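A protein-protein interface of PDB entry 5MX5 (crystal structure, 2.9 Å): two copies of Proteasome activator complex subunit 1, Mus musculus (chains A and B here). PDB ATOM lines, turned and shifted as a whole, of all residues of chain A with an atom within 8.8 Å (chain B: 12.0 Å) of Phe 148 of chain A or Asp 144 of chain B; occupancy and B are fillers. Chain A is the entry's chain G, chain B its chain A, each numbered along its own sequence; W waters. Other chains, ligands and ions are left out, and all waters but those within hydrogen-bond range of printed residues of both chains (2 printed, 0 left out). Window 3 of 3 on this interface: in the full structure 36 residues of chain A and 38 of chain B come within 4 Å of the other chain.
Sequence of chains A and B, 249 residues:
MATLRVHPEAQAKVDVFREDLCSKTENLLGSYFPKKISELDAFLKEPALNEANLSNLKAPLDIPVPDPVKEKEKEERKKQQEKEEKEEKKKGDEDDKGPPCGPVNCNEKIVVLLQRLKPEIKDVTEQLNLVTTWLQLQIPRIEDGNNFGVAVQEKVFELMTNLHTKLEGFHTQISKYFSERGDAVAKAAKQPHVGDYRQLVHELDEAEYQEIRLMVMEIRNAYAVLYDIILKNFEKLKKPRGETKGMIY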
ATOM      1  N   PRO A 140      -3.780  19.837 -13.840  1.00  0.00           N
ATOM      2  CA  PRO A 140      -3.939  19.849 -12.387  1.00  0.00           C
ATOM      3  C   PRO A 140      -5.259  20.483 -11.930  1.00  0.00           C
ATOM      4  O   PRO A 140      -6.111  20.817 -12.760  1.00  0.00           O
ATOM      5  CB  PRO A 140      -2.742  20.686 -11.935  1.00  0.00           C
ATOM      6  CG  PRO A 140      -2.590  21.692 -13.020  1.00  0.00           C
ATOM      7  CD  PRO A 140      -2.987  20.997 -14.297  1.00  0.00           C
ATOM      8  N   GLU A 143      -7.171  26.413 -10.243  1.00  0.00           N
ATOM      9  CA  GLU A 143      -6.770  27.353  -9.190  1.00  0.00           C
ATOM     10  C   GLU A 143      -6.864  28.810  -9.637  1.00  0.00           C
ATOM     11  O   GLU A 143      -6.957  29.112 -10.830  1.00  0.00           O
ATOM     12  CB  GLU A 143      -5.346  27.045  -8.715  1.00  0.00           C
ATOM     13  CG  GLU A 143      -5.222  25.730  -7.959  1.00  0.00           C
ATOM     14  CD  GLU A 143      -3.861  25.535  -7.308  1.00  0.00           C
ATOM     15  OE1 GLU A 143      -2.888  26.216  -7.703  1.00  0.00           O
ATOM     16  OE2 GLU A 143      -3.762  24.687  -6.395  1.00  0.00           O
ATOM     17  N   GLY A 145      -4.610  31.305  -9.303  1.00  0.00           N
ATOM     18  CA  GLY A 145      -3.390  31.757  -9.982  1.00  0.00           C
ATOM     19  C   GLY A 145      -2.432  30.612 -10.251  1.00  0.00           C
ATOM     20  O   GLY A 145      -2.783  29.443 -10.060  1.00  0.00           O
ATOM     21  N   ASN A 146      -1.226  30.959 -10.704  1.00  0.00           N
ATOM     22  CA  ASN A 146      -0.161  29.996 -11.018  1.00  0.00           C
ATOM     23  C   ASN A 146      -0.607  29.052 -12.148  1.00  0.00           C
ATOM     24  O   ASN A 146      -0.440  27.830 -12.070  1.00  0.00           O
ATOM     25  CB  ASN A 146       0.265  29.230  -9.747  1.00  0.00           C
ATOM     26  CG  ASN A 146       1.622  28.551  -9.877  1.00  0.00           C
ATOM     27  OD1 ASN A 146       2.323  28.693 -10.881  1.00  0.00           O
ATOM     28  ND2 ASN A 146       1.997  27.800  -8.849  1.00  0.00           N
ATOM     29  N   ASN A 147      -1.165  29.650 -13.201  1.00  0.00           N
ATOM     30  CA  ASN A 147      -1.794  28.919 -14.304  1.00  0.00           C
ATOM     31  C   ASN A 147      -1.011  29.006 -15.625  1.00  0.00           C
ATOM     32  O   ASN A 147      -1.590  28.802 -16.696  1.00  0.00           O
ATOM     33  CB  ASN A 147      -3.223  29.447 -14.512  1.00  0.00           C
ATOM     34  CG  ASN A 147      -4.153  29.079 -13.375  1.00  0.00           C
ATOM     35  OD1 ASN A 147      -4.586  29.939 -12.606  1.00  0.00           O
ATOM     36  ND2 ASN A 147      -4.474  27.797 -13.267  1.00  0.00           N
ATOM     37  N   PHE A 148       0.295  29.284 -15.564  1.00  0.00           N
ATOM     38  CA  PHE A 148       1.095  29.368 -16.790  1.00  0.00           C
ATOM     39  C   PHE A 148       1.313  27.985 -17.402  1.00  0.00           C
ATOM     40  O   PHE A 148       1.116  27.802 -18.602  1.00  0.00           O
ATOM     41  CB  PHE A 148       2.445  30.058 -16.579  1.00  0.00           C
ATOM     42  CG  PHE A 148       3.255  30.141 -17.842  1.00  0.00           C
ATOM     43  CD1 PHE A 148       2.856  30.985 -18.874  1.00  0.00           C
ATOM     44  CD2 PHE A 148       4.372  29.331 -18.031  1.00  0.00           C
ATOM     45  CE1 PHE A 148       3.575  31.045 -20.058  1.00  0.00           C
ATOM     46  CE2 PHE A 148       5.096  29.390 -19.212  1.00  0.00           C
ATOM     47  CZ  PHE A 148       4.696  30.246 -20.225  1.00  0.00           C
ATOM     48  N   GLY A 149       1.721  27.025 -16.573  1.00  0.00           N
ATOM     49  CA  GLY A 149       1.837  25.625 -16.991  1.00  0.00           C
ATOM     50  C   GLY A 149       0.528  25.033 -17.492  1.00  0.00           C
ATOM     51  O   GLY A 149       0.534  24.166 -18.366  1.00  0.00           O
ATOM     52  N   VAL A 150      -0.590  25.511 -16.943  1.00  0.00           N
ATOM     53  CA  VAL A 150      -1.926  25.137 -17.419  1.00  0.00           C
ATOM     54  C   VAL A 150      -2.174  25.728 -18.815  1.00  0.00           C
ATOM     55  O   VAL A 150      -2.737  25.054 -19.678  1.00  0.00           O
ATOM     56  CB  VAL A 150      -3.037  25.582 -16.432  1.00  0.00           C
ATOM     57  CG1 VAL A 150      -4.421  25.203 -16.959  1.00  0.00           C
ATOM     58  CG2 VAL A 150      -2.802  24.969 -15.051  1.00  0.00           C
ATOM     59  N   ALA A 151      -1.756  26.978 -19.025  1.00  0.00           N
ATOM     60  CA  ALA A 151      -1.823  27.621 -20.347  1.00  0.00           C
ATOM     61  C   ALA A 151      -0.906  26.956 -21.381  1.00  0.00           C
ATOM     62  O   ALA A 151      -1.245  26.912 -22.567  1.00  0.00           O
ATOM     63  CB  ALA A 151      -1.502  29.107 -20.240  1.00  0.00           C
ATOM     64  N   VAL A 152       0.247  26.455 -20.934  1.00  0.00           N
ATOM     65  CA  VAL A 152       1.158  25.677 -21.791  1.00  0.00           C
ATOM     66  C   VAL A 152       0.483  24.383 -22.257  1.00  0.00           C
ATOM     67  O   VAL A 152       0.563  24.033 -23.434  1.00  0.00           O
ATOM     68  CB  VAL A 152       2.501  25.366 -21.074  1.00  0.00           C
ATOM     69  CG1 VAL A 152       3.326  24.320 -21.826  1.00  0.00           C
ATOM     70  CG2 VAL A 152       3.314  26.642 -20.897  1.00  0.00           C
ATOM     71  N   GLN A 153      -0.171  23.683 -21.329  1.00  0.00           N
ATOM     72  CA  GLN A 153      -0.930  22.467 -21.653  1.00  0.00           C
ATOM     73  C   GLN A 153      -2.058  22.737 -22.654  1.00  0.00           C
ATOM     74  O   GLN A 153      -2.253  21.959 -23.586  1.00  0.00           O
ATOM     75  CB  GLN A 153      -1.502  21.828 -20.383  1.00  0.00           C
ATOM     76  CG  GLN A 153      -0.451  21.182 -19.491  1.00  0.00           C
ATOM     77  CD  GLN A 153      -0.983  20.779 -18.128  1.00  0.00           C
ATOM     78  OE1 GLN A 153      -1.911  21.391 -17.594  1.00  0.00           O
ATOM     79  NE2 GLN A 153      -0.386  19.744 -17.549  1.00  0.00           N
ATOM     80  N   GLU A 154      -2.782  23.837 -22.453  1.00  0.00           N
ATOM     81  CA  GLU A 154      -3.859  24.255 -23.364  1.00  0.00           C
ATOM     82  C   GLU A 154      -3.368  24.589 -24.781  1.00  0.00           C
ATOM     83  O   GLU A 154      -4.060  24.288 -25.758  1.00  0.00           O
ATOM     84  CB  GLU A 154      -4.621  25.454 -22.784  1.00  0.00           C
ATOM     85  CG  GLU A 154      -5.496  25.107 -21.584  1.00  0.00           C
ATOM     86  CD  GLU A 154      -6.099  26.324 -20.892  1.00  0.00           C
ATOM     87  OE1 GLU A 154      -5.871  27.469 -21.344  1.00  0.00           O
ATOM     88  OE2 GLU A 154      -6.812  26.133 -19.884  1.00  0.00           O
ATOM     89  N   LYS A 155      -2.191  25.207 -24.886  1.00  0.00           N
ATOM     90  CA  LYS A 155      -1.587  25.542 -26.186  1.00  0.00           C
ATOM     91  C   LYS A 155      -1.139  24.292 -26.953  1.00  0.00           C
ATOM     92  O   LYS A 155      -1.320  24.215 -28.170  1.00  0.00           O
ATOM     93  CB  LYS A 155      -0.401  26.505 -26.001  1.00  0.00           C
ATOM     94  CG  LYS A 155       0.254  26.999 -27.290  1.00  0.00           C
ATOM     95  CD  LYS A 155      -0.595  28.022 -28.030  1.00  0.00           C
ATOM     96  CE  LYS A 155      -0.159  28.152 -29.483  1.00  0.00           C
ATOM     97  NZ  LYS A 155      -0.614  29.427 -30.105  1.00  0.00           N
ATOM     98  N   ASN A 233       8.410  21.483 -24.547  1.00  0.00           N
ATOM     99  CA  ASN A 233       7.569  21.919 -23.424  1.00  0.00           C
ATOM    100  C   ASN A 233       7.351  20.850 -22.335  1.00  0.00           C
ATOM    101  O   ASN A 233       6.538  21.061 -21.433  1.00  0.00           O
ATOM    102  CB  ASN A 233       6.207  22.380 -23.964  1.00  0.00           C
ATOM    103  CG  ASN A 233       6.332  23.511 -24.969  1.00  0.00           C
ATOM    104  OD1 ASN A 233       6.929  24.547 -24.680  1.00  0.00           O
ATOM    105  ND2 ASN A 233       5.762  23.320 -26.154  1.00  0.00           N
ATOM    106  N   LYS A 236       6.931  21.725 -18.436  1.00  0.00           N
ATOM    107  CA  LYS A 236       5.678  22.425 -18.119  1.00  0.00           C
ATOM    108  C   LYS A 236       4.424  21.573 -18.362  1.00  0.00           C
ATOM    109  O   LYS A 236       3.400  21.795 -17.715  1.00  0.00           O
ATOM    110  CB  LYS A 236       5.579  23.745 -18.897  1.00  0.00           C
ATOM    111  CG  LYS A 236       6.535  24.822 -18.405  1.00  0.00           C
ATOM    112  CD  LYS A 236       6.006  25.521 -17.160  1.00  0.00           C
ATOM    113  CE  LYS A 236       6.990  26.545 -16.618  1.00  0.00           C
ATOM    114  NZ  LYS A 236       8.066  25.924 -15.795  1.00  0.00           N
ATOM    115  N   LEU A 237       4.494  20.618 -19.291  1.00  0.00           N
ATOM    116  CA  LEU A 237       3.384  19.682 -19.525  1.00  0.00           C
ATOM    117  C   LEU A 237       3.257  18.662 -18.393  1.00  0.00           C
ATOM    118  O   LEU A 237       2.151  18.404 -17.912  1.00  0.00           O
ATOM    119  CB  LEU A 237       3.549  18.953 -20.862  1.00  0.00           C
ATOM    120  CG  LEU A 237       3.545  19.803 -22.138  1.00  0.00           C
ATOM    121  CD1 LEU A 237       3.979  18.960 -23.329  1.00  0.00           C
ATOM    122  CD2 LEU A 237       2.187  20.434 -22.405  1.00  0.00           C
ATOM    123  N   LYS A 239       5.064  18.776 -15.266  1.00  0.00           N
ATOM    124  CA  LYS A 239       5.017  19.547 -14.018  1.00  0.00           C
ATOM    125  C   LYS A 239       4.537  20.984 -14.298  1.00  0.00           C
ATOM    126  O   LYS A 239       5.363  21.891 -14.446  1.00  0.00           O
ATOM    127  CB  LYS A 239       6.400  19.569 -13.358  1.00  0.00           C
ATOM    128  CG  LYS A 239       6.897  18.214 -12.881  1.00  0.00           C
ATOM    129  CD  LYS A 239       8.311  18.321 -12.331  1.00  0.00           C
ATOM    130  CE  LYS A 239       8.851  16.972 -11.889  1.00  0.00           C
ATOM    131  NZ  LYS A 239      10.238  17.081 -11.357  1.00  0.00           N
ATOM    132  N   PRO A 240       3.205  21.195 -14.383  1.00  0.00           N
ATOM    133  CA  PRO A 240       2.682  22.550 -14.631  1.00  0.00           C
ATOM    134  C   PRO A 240       2.882  23.557 -13.485  1.00  0.00           C
ATOM    135  O   PRO A 240       2.860  24.764 -13.736  1.00  0.00           O
ATOM    136  CB  PRO A 240       1.188  22.312 -14.898  1.00  0.00           C
ATOM    137  CG  PRO A 240       0.880  21.012 -14.249  1.00  0.00           C
ATOM    138  CD  PRO A 240       2.127  20.189 -14.357  1.00  0.00           C
ATOM    139  N   ARG A 241       3.067  23.069 -12.256  1.00  0.00           N
ATOM    140  CA  ARG A 241       3.376  23.925 -11.105  1.00  0.00           C
ATOM    141  C   ARG A 241       4.632  23.450 -10.355  1.00  0.00           C
ATOM    142  O   ARG A 241       4.765  23.682  -9.149  1.00  0.00           O
ATOM    143  CB  ARG A 241       2.174  23.979 -10.154  1.00  0.00           C
ATOM    144  CG  ARG A 241       0.861  24.356 -10.827  1.00  0.00           C
ATOM    145  CD  ARG A 241      -0.115  24.994  -9.850  1.00  0.00           C
ATOM    146  NE  ARG A 241      -1.343  25.443 -10.513  1.00  0.00           N
ATOM    147  CZ  ARG A 241      -2.496  24.770 -10.583  1.00  0.00           C
ATOM    148  NH1 ARG A 241      -2.651  23.568 -10.025  1.00  0.00           N
ATOM    149  NH2 ARG A 241      -3.525  25.315 -11.226  1.00  0.00           N
ATOM    150  N   ILE B 139       8.967  27.185 -33.845  1.00  0.00           N
ATOM    151  CA  ILE B 139       8.247  27.698 -32.671  1.00  0.00           C
ATOM    152  C   ILE B 139       8.969  27.207 -31.406  1.00  0.00           C
ATOM    153  O   ILE B 139       9.061  25.997 -31.187  1.00  0.00           O
ATOM    154  CB  ILE B 139       6.761  27.254 -32.650  1.00  0.00           C
ATOM    155  CG1 ILE B 139       6.005  27.861 -33.841  1.00  0.00           C
ATOM    156  CG2 ILE B 139       6.081  27.670 -31.346  1.00  0.00           C
ATOM    157  CD1 ILE B 139       4.638  27.258 -34.090  1.00  0.00           C
ATOM    158  N   PRO B 140       9.473  28.140 -30.570  1.00  0.00           N
ATOM    159  CA  PRO B 140      10.287  27.758 -29.416  1.00  0.00           C
ATOM    160  C   PRO B 140       9.463  27.252 -28.229  1.00  0.00           C
ATOM    161  O   PRO B 140       8.240  27.112 -28.330  1.00  0.00           O
ATOM    162  CB  PRO B 140      10.994  29.070 -29.061  1.00  0.00           C
ATOM    163  CG  PRO B 140       9.994  30.114 -29.405  1.00  0.00           C
ATOM    164  CD  PRO B 140       9.247  29.599 -30.606  1.00  0.00           C
ATOM    165  N   ARG B 141      10.148  26.969 -27.121  1.00  0.00           N
ATOM    166  CA  ARG B 141       9.502  26.620 -25.852  1.00  0.00           C
ATOM    167  C   ARG B 141       8.604  27.771 -25.393  1.00  0.00           C
ATOM    168  O   ARG B 141       8.956  28.940 -25.558  1.00  0.00           O
ATOM    169  CB  ARG B 141      10.562  26.325 -24.784  1.00  0.00           C
ATOM    170  CG  ARG B 141      10.020  25.845 -23.445  1.00  0.00           C
ATOM    171  CD  ARG B 141      11.154  25.559 -22.473  1.00  0.00           C
ATOM    172  NE  ARG B 141      11.866  26.778 -22.083  1.00  0.00           N
ATOM    173  CZ  ARG B 141      12.977  26.820 -21.343  1.00  0.00           C
ATOM    174  NH1 ARG B 141      13.544  25.704 -20.883  1.00  0.00           N
ATOM    175  NH2 ARG B 141      13.530  27.997 -21.056  1.00  0.00           N
ATOM    176  N   ILE B 142       7.456  27.431 -24.809  1.00  0.00           N
ATOM    177  CA  ILE B 142       6.482  28.436 -24.379  1.00  0.00           C
ATOM    178  C   ILE B 142       6.997  29.050 -23.075  1.00  0.00           C
ATOM    179  O   ILE B 142       7.197  28.340 -22.087  1.00  0.00           O
ATOM    180  CB  ILE B 142       5.062  27.844 -24.192  1.00  0.00           C
ATOM    181  CG1 ILE B 142       4.588  27.153 -25.482  1.00  0.00           C
ATOM    182  CG2 ILE B 142       4.060  28.934 -23.811  1.00  0.00           C
ATOM    183  CD1 ILE B 142       3.254  26.447 -25.362  1.00  0.00           C
ATOM    184  N   GLU B 143       7.213  30.366 -23.098  1.00  0.00           N
ATOM    185  CA  GLU B 143       7.769  31.118 -21.970  1.00  0.00           C
ATOM    186  C   GLU B 143       6.869  32.305 -21.639  1.00  0.00           C
ATOM    187  O   GLU B 143       6.109  32.779 -22.488  1.00  0.00           O
ATOM    188  CB  GLU B 143       9.187  31.596 -22.289  1.00  0.00           C
ATOM    189  CG  GLU B 143      10.210  30.469 -22.381  1.00  0.00           C
ATOM    190  CD  GLU B 143      11.634  30.953 -22.621  1.00  0.00           C
ATOM    191  OE1 GLU B 143      11.853  32.174 -22.787  1.00  0.00           O
ATOM    192  OE2 GLU B 143      12.545  30.099 -22.646  1.00  0.00           O
ATOM    193  N   ASP B 144       6.962  32.768 -20.395  1.00  0.00           N
ATOM    194  CA  ASP B 144       6.021  33.752 -19.847  1.00  0.00           C
ATOM    195  C   ASP B 144       6.137  35.135 -20.500  1.00  0.00           C
ATOM    196  O   ASP B 144       5.132  35.834 -20.648  1.00  0.00           O
ATOM    197  CB  ASP B 144       6.204  33.863 -18.324  1.00  0.00           C
ATOM    198  CG  ASP B 144       5.021  34.530 -17.622  1.00  0.00           C
ATOM    199  OD1 ASP B 144       3.918  34.618 -18.203  1.00  0.00           O
ATOM    200  OD2 ASP B 144       5.204  34.964 -16.463  1.00  0.00           O
ATOM    201  N   GLY B 145       7.356  35.518 -20.884  1.00  0.00           N
ATOM    202  CA  GLY B 145       7.609  36.774 -21.597  1.00  0.00           C
ATOM    203  C   GLY B 145       8.500  36.584 -22.811  1.00  0.00           C
ATOM    204  O   GLY B 145       8.931  35.466 -23.108  1.00  0.00           O
ATOM    205  N   ASN B 146       8.757  37.691 -23.510  1.00  0.00           N
ATOM    206  CA  ASN B 146       9.589  37.732 -24.721  1.00  0.00           C
ATOM    207  C   ASN B 146       8.932  36.921 -25.850  1.00  0.00           C
ATOM    208  O   ASN B 146       9.562  36.064 -26.477  1.00  0.00           O
ATOM    209  CB  ASN B 146      11.027  37.261 -24.415  1.00  0.00           C
ATOM    210  CG  ASN B 146      12.039  37.689 -25.472  1.00  0.00           C
ATOM    211  OD1 ASN B 146      11.717  38.399 -26.427  1.00  0.00           O
ATOM    212  ND2 ASN B 146      13.281  37.250 -25.301  1.00  0.00           N
ATOM    213  N   ASN B 147       7.655  37.221 -26.097  1.00  0.00           N
ATOM    214  CA  ASN B 147       6.826  36.484 -27.057  1.00  0.00           C
ATOM    215  C   ASN B 147       6.452  37.315 -28.294  1.00  0.00           C
ATOM    216  O   ASN B 147       5.430  37.044 -28.934  1.00  0.00           O
ATOM    217  CB  ASN B 147       5.554  35.981 -26.359  1.00  0.00           C
ATOM    218  CG  ASN B 147       5.851  35.055 -25.194  1.00  0.00           C
ATOM    219  OD1 ASN B 147       6.645  34.122 -25.315  1.00  0.00           O
ATOM    220  ND2 ASN B 147       5.203  35.303 -24.060  1.00  0.00           N
ATOM    221  N   PHE B 148       7.273  38.308 -28.641  1.00  0.00           N
ATOM    222  CA  PHE B 148       7.043  39.099 -29.856  1.00  0.00           C
ATOM    223  C   PHE B 148       7.422  38.302 -31.105  1.00  0.00           C
ATOM    224  O   PHE B 148       6.691  38.320 -32.095  1.00  0.00           O
ATOM    225  CB  PHE B 148       7.805  40.426 -29.828  1.00  0.00           C
ATOM    226  CG  PHE B 148       7.598  41.254 -31.065  1.00  0.00           C
ATOM    227  CD1 PHE B 148       6.354  41.819 -31.334  1.00  0.00           C
ATOM    228  CD2 PHE B 148       8.630  41.439 -31.984  1.00  0.00           C
ATOM    229  CE1 PHE B 148       6.146  42.569 -32.483  1.00  0.00           C
ATOM    230  CE2 PHE B 148       8.428  42.189 -33.135  1.00  0.00           C
ATOM    231  CZ  PHE B 148       7.186  42.754 -33.384  1.00  0.00           C
ATOM    232  N   GLY B 149       8.564  37.616 -31.053  1.00  0.00           N
ATOM    233  CA  GLY B 149       8.985  36.704 -32.123  1.00  0.00           C
ATOM    234  C   GLY B 149       8.023  35.547 -32.351  1.00  0.00           C
ATOM    235  O   GLY B 149       7.851  35.096 -33.484  1.00  0.00           O
ATOM    236  N   VAL B 150       7.399  35.075 -31.271  1.00  0.00           N
ATOM    237  CA  VAL B 150       6.347  34.055 -31.348  1.00  0.00           C
ATOM    238  C   VAL B 150       5.117  34.619 -32.074  1.00  0.00           C
ATOM    239  O   VAL B 150       4.498  33.918 -32.878  1.00  0.00           O
ATOM    240  CB  VAL B 150       5.962  33.524 -29.940  1.00  0.00           C
ATOM    241  CG1 VAL B 150       4.750  32.595 -30.001  1.00  0.00           C
ATOM    242  CG2 VAL B 150       7.145  32.803 -29.301  1.00  0.00           C
ATOM    243  N   ALA B 151       4.773  35.876 -31.784  1.00  0.00           N
ATOM    244  CA  ALA B 151       3.670  36.569 -32.465  1.00  0.00           C
ATOM    245  C   ALA B 151       3.932  36.799 -33.958  1.00  0.00           C
ATOM    246  O   ALA B 151       2.991  36.787 -34.755  1.00  0.00           O
ATOM    247  CB  ALA B 151       3.362  37.894 -31.777  1.00  0.00           C
ATOM    248  N   GLU B 154       3.320  33.361 -35.539  1.00  0.00           N
ATOM    249  CA  GLU B 154       1.862  33.168 -35.607  1.00  0.00           C
ATOM    250  C   GLU B 154       1.190  34.007 -36.700  1.00  0.00           C
ATOM    251  O   GLU B 154       0.245  33.542 -37.338  1.00  0.00           O
ATOM    252  CB  GLU B 154       1.207  33.466 -34.252  1.00  0.00           C
ATOM    253  CG  GLU B 154       1.463  32.397 -33.198  1.00  0.00           C
ATOM    254  CD  GLU B 154       0.983  32.790 -31.809  1.00  0.00           C
ATOM    255  OE1 GLU B 154       0.169  33.732 -31.686  1.00  0.00           O
ATOM    256  OE2 GLU B 154       1.420  32.146 -30.829  1.00  0.00           O
ATOM    257  N   ARG B 241      13.786  34.743 -30.388  1.00  0.00           N
ATOM    258  CA  ARG B 241      14.332  35.362 -29.170  1.00  0.00           C
ATOM    259  C   ARG B 241      15.815  35.764 -29.297  1.00  0.00           C
ATOM    260  O   ARG B 241      16.517  35.893 -28.290  1.00  0.00           O
ATOM    261  CB  ARG B 241      14.102  34.421 -27.979  1.00  0.00           C
ATOM    262  CG  ARG B 241      12.654  34.414 -27.513  1.00  0.00           C
ATOM    263  CD  ARG B 241      12.272  33.142 -26.779  1.00  0.00           C
ATOM    264  NE  ARG B 241      10.830  33.092 -26.538  1.00  0.00           N
ATOM    265  CZ  ARG B 241      10.162  32.036 -26.071  1.00  0.00           C
ATOM    266  NH1 ARG B 241      10.788  30.897 -25.772  1.00  0.00           N
ATOM    267  NH2 ARG B 241       8.844  32.120 -25.903  1.00  0.00           N
HETATM  268  O   HOH W   1       6.830  25.172 -21.934  1.00  0.00           O
HETATM  269  O   HOH W   2       6.374  25.055 -28.686  1.00  0.00           O
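Water W2 bridges the backbone carbonyl oxygen of Pro 140 of chain B and the side-chain amide nitrogen of Asn 233 of chain A.
Water W1 lies within hydrogen-bond range of OD1 of Asn 233 of chain A (2.8 Å) and O of Ile 142 of chain B (3.2 Å).
Hydrophobic or aromatic side chains of chain A that line the printed part of chain B: Phe 148 and Val 152.
Hydrophobic or aromatic side chains of chain B that line the printed part of chain A: Ile 142.
Among the printed residues, 8 pairs touch across the chains.
Among the printed residues, Asp or Glu carboxylates within 4 Å of a Lys or Arg side-chain nitrogen of the other chain: Lys 155 of chain A with Glu 154 of chain B (3.5 Å).
Phe 148 of chain A touches Glu 143 of chain B, but with the chains exchanged Glu 143 of chain A does not touch Phe 148 of chain B (24.6 Å).
11 positions are printed for both chains.
Of the 8 pairs that touch across the chains among the printed residues, none has its exchanged pair printed and touching as well.
No residue of chain B comes within 4 Å of Asn 147 of chain A.
Phe 148 of chain A touches three residues of chain B.
No residue of chain B comes within 4 Å of Gly 149 of chain A.
No residue of chain B comes within 4 Å of Val 150 of chain A.
No residue of chain B comes within 4 Å of Ala 151 of chain A.
Val 152 of chain A touches just one residue of chain B: Ile 142.
Of the printed residues of chain B, Lys 155 of chain A touches Ile 142 and Glu 154.
Of the printed residues of chain B, Asn 233 of chain A touches Arg 141 (3.5 Å) and Ile 142 (2.9 Å).
No residue of chain B comes within 4 Å of Lys 236 of chain A.
Arg 241 of chain A touches none of the printed residues of chain B.
Printed residues of chain A within 4 Å of Ile 142 of chain B: Phe 148, Val 152, Lys 155 and Asn 233.
Of the printed residues of chain A, Glu 143 of chain B touches Phe 148.
Of chain A, only Phe 148 (3.4 Å) comes within 4 Å of Asp 144 of chain B.
Val 150 of chain B touches none of the printed residues of chain A.
The nearest residue of chain B that does not touch Phe 148 of chain A is Gly 145 of chain B (5.9 Å).
The nearest printed residue of chain A that does not touch Glu 143 of chain B is Val 152 of chain A (5.8 Å).
The guanidinium group of Arg 241 of chain B is in hydrogen-bond range of the backbone carbonyl oxygen of Arg 141 of chain B, 2.7 Å away.
O of Asp 144 of chain B lies within hydrogen-bond range of ND2 of Asn 147 of chain B (3.5 Å).
The side-chain carboxylate (OE2) of Glu 143 of chain B lies within salt-bridge range of the guanidinium group (NH2) of Arg 141 of chain B, 2.8 Å away.
O of Glu 143 of chain B lies within hydrogen-bond range of ND2 of Asn 147 of chain B.
The side-chain carboxylate of Glu 143 of chain B lies within salt-bridge range of the guanidinium group of Arg 241 of chain B (3.4 Å).
NZ of Lys 155 of chain A is in salt-bridge range of OE2 of Glu 154 of chain B, at 3.5 Å.
The backbone NH (N) of Ile 142 of chain B lies within hydrogen-bond range of the side-chain amide oxygen (OD1) of Asn 233 of chain A (2.9 Å).
CZ of Phe 148 of chain A touches O of Ile 142 of chain B, 3.7 Å away.
Glu 143 of chain B touches Phe 148 of chain A (C to CZ, 3.3 Å).
N of Asp 144 of chain B touches CZ of Phe 148 of chain A (3.4 Å).
CG2 of Val 152 of chain A touches CG2 of Ile 142 of chain B (3.8 Å).
Ile 142 of chain B touches Lys 155 of chain A (CD1 to CG, 3.6 Å).
Asn 233 of chain A touches Arg 141 of chain B.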
